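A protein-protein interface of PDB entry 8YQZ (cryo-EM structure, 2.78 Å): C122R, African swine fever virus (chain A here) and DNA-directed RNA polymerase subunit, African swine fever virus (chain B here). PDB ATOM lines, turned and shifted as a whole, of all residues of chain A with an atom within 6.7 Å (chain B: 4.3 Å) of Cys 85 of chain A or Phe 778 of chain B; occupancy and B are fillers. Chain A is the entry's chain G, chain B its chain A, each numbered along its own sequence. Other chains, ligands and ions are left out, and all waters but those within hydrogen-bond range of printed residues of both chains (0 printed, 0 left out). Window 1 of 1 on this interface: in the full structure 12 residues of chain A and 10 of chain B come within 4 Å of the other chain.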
ATOM      1  N   PHE A  56     -15.633  -9.089  16.927  1.00  0.00           N
ATOM      2  CA  PHE A  56     -16.456  -8.782  18.090  1.00  0.00           C
ATOM      3  C   PHE A  56     -16.330  -7.321  18.486  1.00  0.00           C
ATOM      4  O   PHE A  56     -17.328  -6.675  18.818  1.00  0.00           O
ATOM      5  CB  PHE A  56     -16.086  -9.679  19.268  1.00  0.00           C
ATOM      6  CG  PHE A  56     -16.742  -9.273  20.549  1.00  0.00           C
ATOM      7  CD1 PHE A  56     -18.084  -9.525  20.763  1.00  0.00           C
ATOM      8  CD2 PHE A  56     -16.028  -8.622  21.535  1.00  0.00           C
ATOM      9  CE1 PHE A  56     -18.696  -9.138  21.929  1.00  0.00           C
ATOM     10  CE2 PHE A  56     -16.640  -8.233  22.707  1.00  0.00           C
ATOM     11  CZ  PHE A  56     -17.972  -8.494  22.903  1.00  0.00           C
ATOM     12  N   THR A  65     -26.809  -6.404  23.883  1.00  0.00           N
ATOM     13  CA  THR A  65     -26.583  -7.063  25.153  1.00  0.00           C
ATOM     14  C   THR A  65     -25.265  -6.665  25.790  1.00  0.00           C
ATOM     15  O   THR A  65     -24.810  -7.345  26.711  1.00  0.00           O
ATOM     16  CB  THR A  65     -26.629  -8.577  24.968  1.00  0.00           C
ATOM     17  OG1 THR A  65     -25.421  -9.021  24.347  1.00  0.00           O
ATOM     18  CG2 THR A  65     -27.778  -8.949  24.093  1.00  0.00           C
ATOM     19  N   ASN A  66     -24.637  -5.599  25.310  1.00  0.00           N
ATOM     20  CA  ASN A  66     -23.360  -5.138  25.829  1.00  0.00           C
ATOM     21  C   ASN A  66     -23.569  -4.009  26.826  1.00  0.00           C
ATOM     22  O   ASN A  66     -24.484  -3.195  26.689  1.00  0.00           O
ATOM     23  CB  ASN A  66     -22.451  -4.668  24.691  1.00  0.00           C
ATOM     24  CG  ASN A  66     -21.697  -5.804  24.038  1.00  0.00           C
ATOM     25  OD1 ASN A  66     -21.326  -6.771  24.686  1.00  0.00           O
ATOM     26  ND2 ASN A  66     -21.467  -5.690  22.745  1.00  0.00           N
ATOM     27  N   CYS A  67     -22.703  -3.967  27.836  1.00  0.00           N
ATOM     28  CA  CYS A  67     -22.778  -2.961  28.887  1.00  0.00           C
ATOM     29  C   CYS A  67     -22.455  -1.581  28.326  1.00  0.00           C
ATOM     30  O   CYS A  67     -21.564  -1.439  27.487  1.00  0.00           O
ATOM     31  CB  CYS A  67     -21.815  -3.316  30.016  1.00  0.00           C
ATOM     32  SG  CYS A  67     -21.835  -2.170  31.392  1.00  0.00           S
ATOM     33  N   GLN A  83     -18.766  -0.229  26.640  1.00  0.00           N
ATOM     34  CA  GLN A  83     -17.551  -0.703  27.281  1.00  0.00           C
ATOM     35  C   GLN A  83     -17.474  -2.219  27.200  1.00  0.00           C
ATOM     36  O   GLN A  83     -18.496  -2.903  27.284  1.00  0.00           O
ATOM     37  CB  GLN A  83     -17.491  -0.229  28.731  1.00  0.00           C
ATOM     38  CG  GLN A  83     -18.293  -1.037  29.717  1.00  0.00           C
ATOM     39  CD  GLN A  83     -17.416  -1.809  30.666  1.00  0.00           C
ATOM     40  OE1 GLN A  83     -16.323  -1.364  31.008  1.00  0.00           O
ATOM     41  NE2 GLN A  83     -17.884  -2.973  31.097  1.00  0.00           N
ATOM     42  N   ILE A  84     -16.269  -2.738  27.001  1.00  0.00           N
ATOM     43  CA  ILE A  84     -16.020  -4.170  26.969  1.00  0.00           C
ATOM     44  C   ILE A  84     -14.769  -4.450  27.784  1.00  0.00           C
ATOM     45  O   ILE A  84     -13.976  -3.542  28.047  1.00  0.00           O
ATOM     46  CB  ILE A  84     -15.876  -4.707  25.530  1.00  0.00           C
ATOM     47  CG1 ILE A  84     -14.885  -3.865  24.733  1.00  0.00           C
ATOM     48  CG2 ILE A  84     -17.219  -4.696  24.829  1.00  0.00           C
ATOM     49  CD1 ILE A  84     -14.943  -4.093  23.244  1.00  0.00           C
ATOM     50  N   CYS A  85     -14.607  -5.695  28.210  1.00  0.00           N
ATOM     51  CA  CYS A  85     -13.516  -6.107  29.086  1.00  0.00           C
ATOM     52  C   CYS A  85     -13.082  -7.511  28.683  1.00  0.00           C
ATOM     53  O   CYS A  85     -13.564  -8.501  29.231  1.00  0.00           O
ATOM     54  CB  CYS A  85     -13.956  -6.045  30.536  1.00  0.00           C
ATOM     55  SG  CYS A  85     -12.730  -6.563  31.727  1.00  0.00           S
ATOM     56  N   ILE A  86     -12.141  -7.596  27.750  1.00  0.00           N
ATOM     57  CA  ILE A  86     -11.760  -8.866  27.147  1.00  0.00           C
ATOM     58  C   ILE A  86     -10.423  -9.327  27.703  1.00  0.00           C
ATOM     59  O   ILE A  86      -9.531  -8.526  27.994  1.00  0.00           O
ATOM     60  CB  ILE A  86     -11.695  -8.768  25.610  1.00  0.00           C
ATOM     61  CG1 ILE A  86     -11.125  -7.414  25.192  1.00  0.00           C
ATOM     62  CG2 ILE A  86     -13.065  -8.983  25.004  1.00  0.00           C
ATOM     63  CD1 ILE A  86     -10.520  -7.408  23.807  1.00  0.00           C
ATOM     64  N   GLY A  87     -10.293 -10.640  27.848  1.00  0.00           N
ATOM     65  CA  GLY A  87      -9.030 -11.252  28.192  1.00  0.00           C
ATOM     66  C   GLY A  87      -8.790 -11.343  29.685  1.00  0.00           C
ATOM     67  O   GLY A  87      -9.521 -10.803  30.510  1.00  0.00           O
ATOM     68  N   GLN A  89      -6.249 -10.076  31.173  1.00  0.00           N
ATOM     69  CA  GLN A  89      -5.725  -8.818  31.674  1.00  0.00           C
ATOM     70  C   GLN A  89      -6.811  -7.773  31.855  1.00  0.00           C
ATOM     71  O   GLN A  89      -6.519  -6.684  32.358  1.00  0.00           O
ATOM     72  CB  GLN A  89      -4.633  -8.294  30.743  1.00  0.00           C
ATOM     73  CG  GLN A  89      -3.383  -9.161  30.769  1.00  0.00           C
ATOM     74  CD  GLN A  89      -2.805  -9.293  32.165  1.00  0.00           C
ATOM     75  OE1 GLN A  89      -2.643  -8.305  32.875  1.00  0.00           O
ATOM     76  NE2 GLN A  89      -2.511 -10.522  32.572  1.00  0.00           N
ATOM     77  N   LYS A  90      -8.046  -8.086  31.474  1.00  0.00           N
ATOM     78  CA  LYS A  90      -9.189  -7.204  31.659  1.00  0.00           C
ATOM     79  C   LYS A  90      -8.917  -5.828  31.064  1.00  0.00           C
ATOM     80  O   LYS A  90      -8.974  -4.801  31.740  1.00  0.00           O
ATOM     81  CB  LYS A  90      -9.563  -7.100  33.137  1.00  0.00           C
ATOM     82  CG  LYS A  90      -9.659  -8.435  33.849  1.00  0.00           C
ATOM     83  CD  LYS A  90     -10.377  -8.298  35.172  1.00  0.00           C
ATOM     84  CE  LYS A  90     -11.688  -7.552  35.022  1.00  0.00           C
ATOM     85  NZ  LYS A  90     -12.862  -8.460  35.041  1.00  0.00           N
ATOM     86  N   ILE A  91      -8.607  -5.825  29.776  1.00  0.00           N
ATOM     87  CA  ILE A  91      -8.442  -4.577  29.048  1.00  0.00           C
ATOM     88  C   ILE A  91      -9.811  -3.942  28.872  1.00  0.00           C
ATOM     89  O   ILE A  91     -10.763  -4.603  28.448  1.00  0.00           O
ATOM     90  CB  ILE A  91      -7.764  -4.811  27.689  1.00  0.00           C
ATOM     91  CG1 ILE A  91      -6.458  -5.586  27.851  1.00  0.00           C
ATOM     92  CG2 ILE A  91      -7.496  -3.493  27.005  1.00  0.00           C
ATOM     93  CD1 ILE A  91      -6.515  -6.986  27.310  1.00  0.00           C
ATOM     94  N   ILE A  92      -9.915  -2.664  29.199  1.00  0.00           N
ATOM     95  CA  ILE A  92     -11.160  -1.924  29.063  1.00  0.00           C
ATOM     96  C   ILE A  92     -11.102  -1.130  27.770  1.00  0.00           C
ATOM     97  O   ILE A  92     -10.203  -0.304  27.579  1.00  0.00           O
ATOM     98  CB  ILE A  92     -11.395  -1.007  30.272  1.00  0.00           C
ATOM     99  CG1 ILE A  92     -11.525  -1.845  31.541  1.00  0.00           C
ATOM    100  CG2 ILE A  92     -12.636  -0.170  30.071  1.00  0.00           C
ATOM    101  CD1 ILE A  92     -12.790  -2.664  31.612  1.00  0.00           C
ATOM    102  N   ILE A  93     -12.055  -1.383  26.878  1.00  0.00           N
ATOM    103  CA  ILE A  93     -12.136  -0.712  25.589  1.00  0.00           C
ATOM    104  C   ILE A  93     -13.489  -0.031  25.489  1.00  0.00           C
ATOM    105  O   ILE A  93     -14.520  -0.660  25.734  1.00  0.00           O
ATOM    106  CB  ILE A  93     -11.949  -1.692  24.416  1.00  0.00           C
ATOM    107  CG1 ILE A  93     -10.700  -2.547  24.607  1.00  0.00           C
ATOM    108  CG2 ILE A  93     -11.882  -0.947  23.107  1.00  0.00           C
ATOM    109  CD1 ILE A  93     -10.603  -3.686  23.626  1.00  0.00           C
ATOM    110  N   PHE B 768     -20.504 -16.016  26.869  1.00  0.00           N
ATOM    111  CA  PHE B 768     -19.290 -15.197  26.751  1.00  0.00           C
ATOM    112  C   PHE B 768     -19.417 -13.870  27.506  1.00  0.00           C
ATOM    113  O   PHE B 768     -19.563 -12.798  26.929  1.00  0.00           O
ATOM    114  CB  PHE B 768     -18.920 -14.937  25.285  1.00  0.00           C
ATOM    115  CG  PHE B 768     -17.743 -14.014  25.119  1.00  0.00           C
ATOM    116  CD1 PHE B 768     -16.504 -14.351  25.625  1.00  0.00           C
ATOM    117  CD2 PHE B 768     -17.887 -12.794  24.487  1.00  0.00           C
ATOM    118  CE1 PHE B 768     -15.438 -13.499  25.497  1.00  0.00           C
ATOM    119  CE2 PHE B 768     -16.820 -11.940  24.357  1.00  0.00           C
ATOM    120  CZ  PHE B 768     -15.598 -12.295  24.859  1.00  0.00           C
ATOM    121  N   GLY B 769     -19.401 -13.975  28.825  1.00  0.00           N
ATOM    122  CA  GLY B 769     -19.318 -12.799  29.657  1.00  0.00           C
ATOM    123  C   GLY B 769     -20.613 -12.344  30.267  1.00  0.00           C
ATOM    124  O   GLY B 769     -20.636 -11.277  30.887  1.00  0.00           O
ATOM    125  N   PRO B 776     -26.286  -7.620  31.413  1.00  0.00           N
ATOM    126  CA  PRO B 776     -25.538  -7.379  30.176  1.00  0.00           C
ATOM    127  C   PRO B 776     -24.196  -8.089  30.185  1.00  0.00           C
ATOM    128  O   PRO B 776     -23.728  -8.607  31.196  1.00  0.00           O
ATOM    129  CB  PRO B 776     -25.374  -5.861  30.153  1.00  0.00           C
ATOM    130  CG  PRO B 776     -25.485  -5.452  31.544  1.00  0.00           C
ATOM    131  CD  PRO B 776     -26.432  -6.392  32.206  1.00  0.00           C
ATOM    132  N   ARG B 777     -23.585  -8.128  29.011  1.00  0.00           N
ATOM    133  CA  ARG B 777     -22.253  -8.693  28.873  1.00  0.00           C
ATOM    134  C   ARG B 777     -21.215  -7.768  29.492  1.00  0.00           C
ATOM    135  O   ARG B 777     -21.302  -6.544  29.368  1.00  0.00           O
ATOM    136  CB  ARG B 777     -21.944  -8.926  27.401  1.00  0.00           C
ATOM    137  CG  ARG B 777     -21.094 -10.136  27.133  1.00  0.00           C
ATOM    138  CD  ARG B 777     -20.449 -10.054  25.763  1.00  0.00           C
ATOM    139  NE  ARG B 777     -21.433 -10.037  24.690  1.00  0.00           N
ATOM    140  CZ  ARG B 777     -22.153 -11.083  24.313  1.00  0.00           C
ATOM    141  NH1 ARG B 777     -22.028 -12.260  24.902  1.00  0.00           N
ATOM    142  NH2 ARG B 777     -23.023 -10.944  23.319  1.00  0.00           N
ATOM    143  N   PHE B 778     -20.220  -8.362  30.149  1.00  0.00           N
ATOM    144  CA  PHE B 778     -19.171  -7.619  30.855  1.00  0.00           C
ATOM    145  C   PHE B 778     -19.767  -6.658  31.875  1.00  0.00           C
ATOM    146  O   PHE B 778     -19.344  -5.509  31.997  1.00  0.00           O
ATOM    147  CB  PHE B 778     -18.256  -6.869  29.883  1.00  0.00           C
ATOM    148  CG  PHE B 778     -17.770  -7.706  28.757  1.00  0.00           C
ATOM    149  CD1 PHE B 778     -17.104  -8.883  28.998  1.00  0.00           C
ATOM    150  CD2 PHE B 778     -18.006  -7.330  27.459  1.00  0.00           C
ATOM    151  CE1 PHE B 778     -16.679  -9.658  27.970  1.00  0.00           C
ATOM    152  CE2 PHE B 778     -17.583  -8.103  26.433  1.00  0.00           C
ATOM    153  CZ  PHE B 778     -16.917  -9.267  26.685  1.00  0.00           C
ATOM    154  N   ALA B 779     -20.769  -7.128  32.607  1.00  0.00           N
ATOM    155  CA  ALA B 779     -21.391  -6.308  33.634  1.00  0.00           C
ATOM    156  C   ALA B 779     -20.453  -6.154  34.820  1.00  0.00           C
ATOM    157  O   ALA B 779     -19.675  -7.057  35.136  1.00  0.00           O
ATOM    158  CB  ALA B 779     -22.712  -6.927  34.077  1.00  0.00           C
ATOM    159  N   LEU B 780     -20.524  -4.998  35.477  1.00  0.00           N
ATOM    160  CA  LEU B 780     -19.634  -4.700  36.589  1.00  0.00           C
ATOM    161  C   LEU B 780     -20.299  -4.793  37.950  1.00  0.00           C
ATOM    162  O   LEU B 780     -19.595  -4.981  38.943  1.00  0.00           O
ATOM    163  CB  LEU B 780     -19.033  -3.300  36.433  1.00  0.00           C
ATOM    164  CG  LEU B 780     -18.292  -3.009  35.136  1.00  0.00           C
ATOM    165  CD1 LEU B 780     -18.536  -1.579  34.706  1.00  0.00           C
ATOM    166  CD2 LEU B 780     -16.814  -3.288  35.303  1.00  0.00           C
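Among the printed residues, pairs that only touch across the chains: Phe 56 of chain A with Phe 768 of chain B, Phe 56 of chain A with Arg 777 of chain B, Phe 56 of chain A with Phe 778 of chain B, Thr 65 of chain A with Pro 776 of chain B, Cys 67 of chain A with Phe 778 of chain B, Gln 83 of chain A with Leu 780 of chain B, Ile 84 of chain A with Phe 778 of chain B and Cys 85 of chain A with Phe 778 of chain B.
The side-chain amide oxygen (OD1) of Asn 66 of chain A is in hydrogen-bond range of the guanidinium group (NE) of Arg 777 of chain B (3.3 Å). The backbone NH (N) of Cys 67 of chain A lies within hydrogen-bond range of the backbone carbonyl oxygen (O) of Arg 777 of chain B. O of Phe 778 of chain B lies within hydrogen-bond range of NE2 of Gln 83 of chain A (3.1 Å). The backbone NH (N) of Arg 777 of chain B lies within hydrogen-bond range of the backbone carbonyl oxygen (O) of Thr 65 of chain A.
The backbone carbonyl oxygen (O) of Cys 67 of chain A is in hydrogen-bond range of the backbone NH (N) of Gln 83 of chain A (3.2 Å). The backbone NH (N) of Phe 778 of chain B is in hydrogen-bond range of the backbone carbonyl oxygen (O) of Gly 769 of chain B, at 3.0 Å. N of Ile 84 of chain A lies within hydrogen-bond range of O of Ile 93 of chain A, 3.0 Å away. O of Phe 768 of chain B sits close to NH1 of Arg 777 of chain B (3.2 Å).
Of the 7 printed residues of chain B, 5 touch a printed residue of chain A. Hydrophobic or aromatic side chains of chain B that line the printed part of chain A: Phe 768, Pro 776, Phe 778 and Leu 780. Of the 14 printed residues of chain A, 7 touch a printed residue of chain B. Among the printed residues, no Asp or Glu carboxylate lies within 4 Å of a Lys or Arg side-chain nitrogen of the other chain.
Of chain B, only Phe 778 comes within 4 Å of Cys 85 of chain A. Phe 778 of chain B touches just these residues of chain A: Phe 56 (3.6 Å), Cys 67 (3.9 Å), Gln 83 (3.1 Å), Ile 84 (3.8 Å) and Cys 85 (3.6 Å). Of the printed residues of chain B, Asn 66 of chain A touches Arg 777 (3.3 Å). Printed residues of chain A within 4 Å of Phe 768 of chain B: Phe 56 (3.9 Å). Lys 90 of chain A touches none of the printed residues of chain B. The nearest printed residue of chain B that does not touch Cys 85 of chain A is Phe 768 of chain B (6.1 Å). The nearest residue of chain A that does not touch Phe 778 of chain B is Ile 86 of chain A (4.2 Å).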
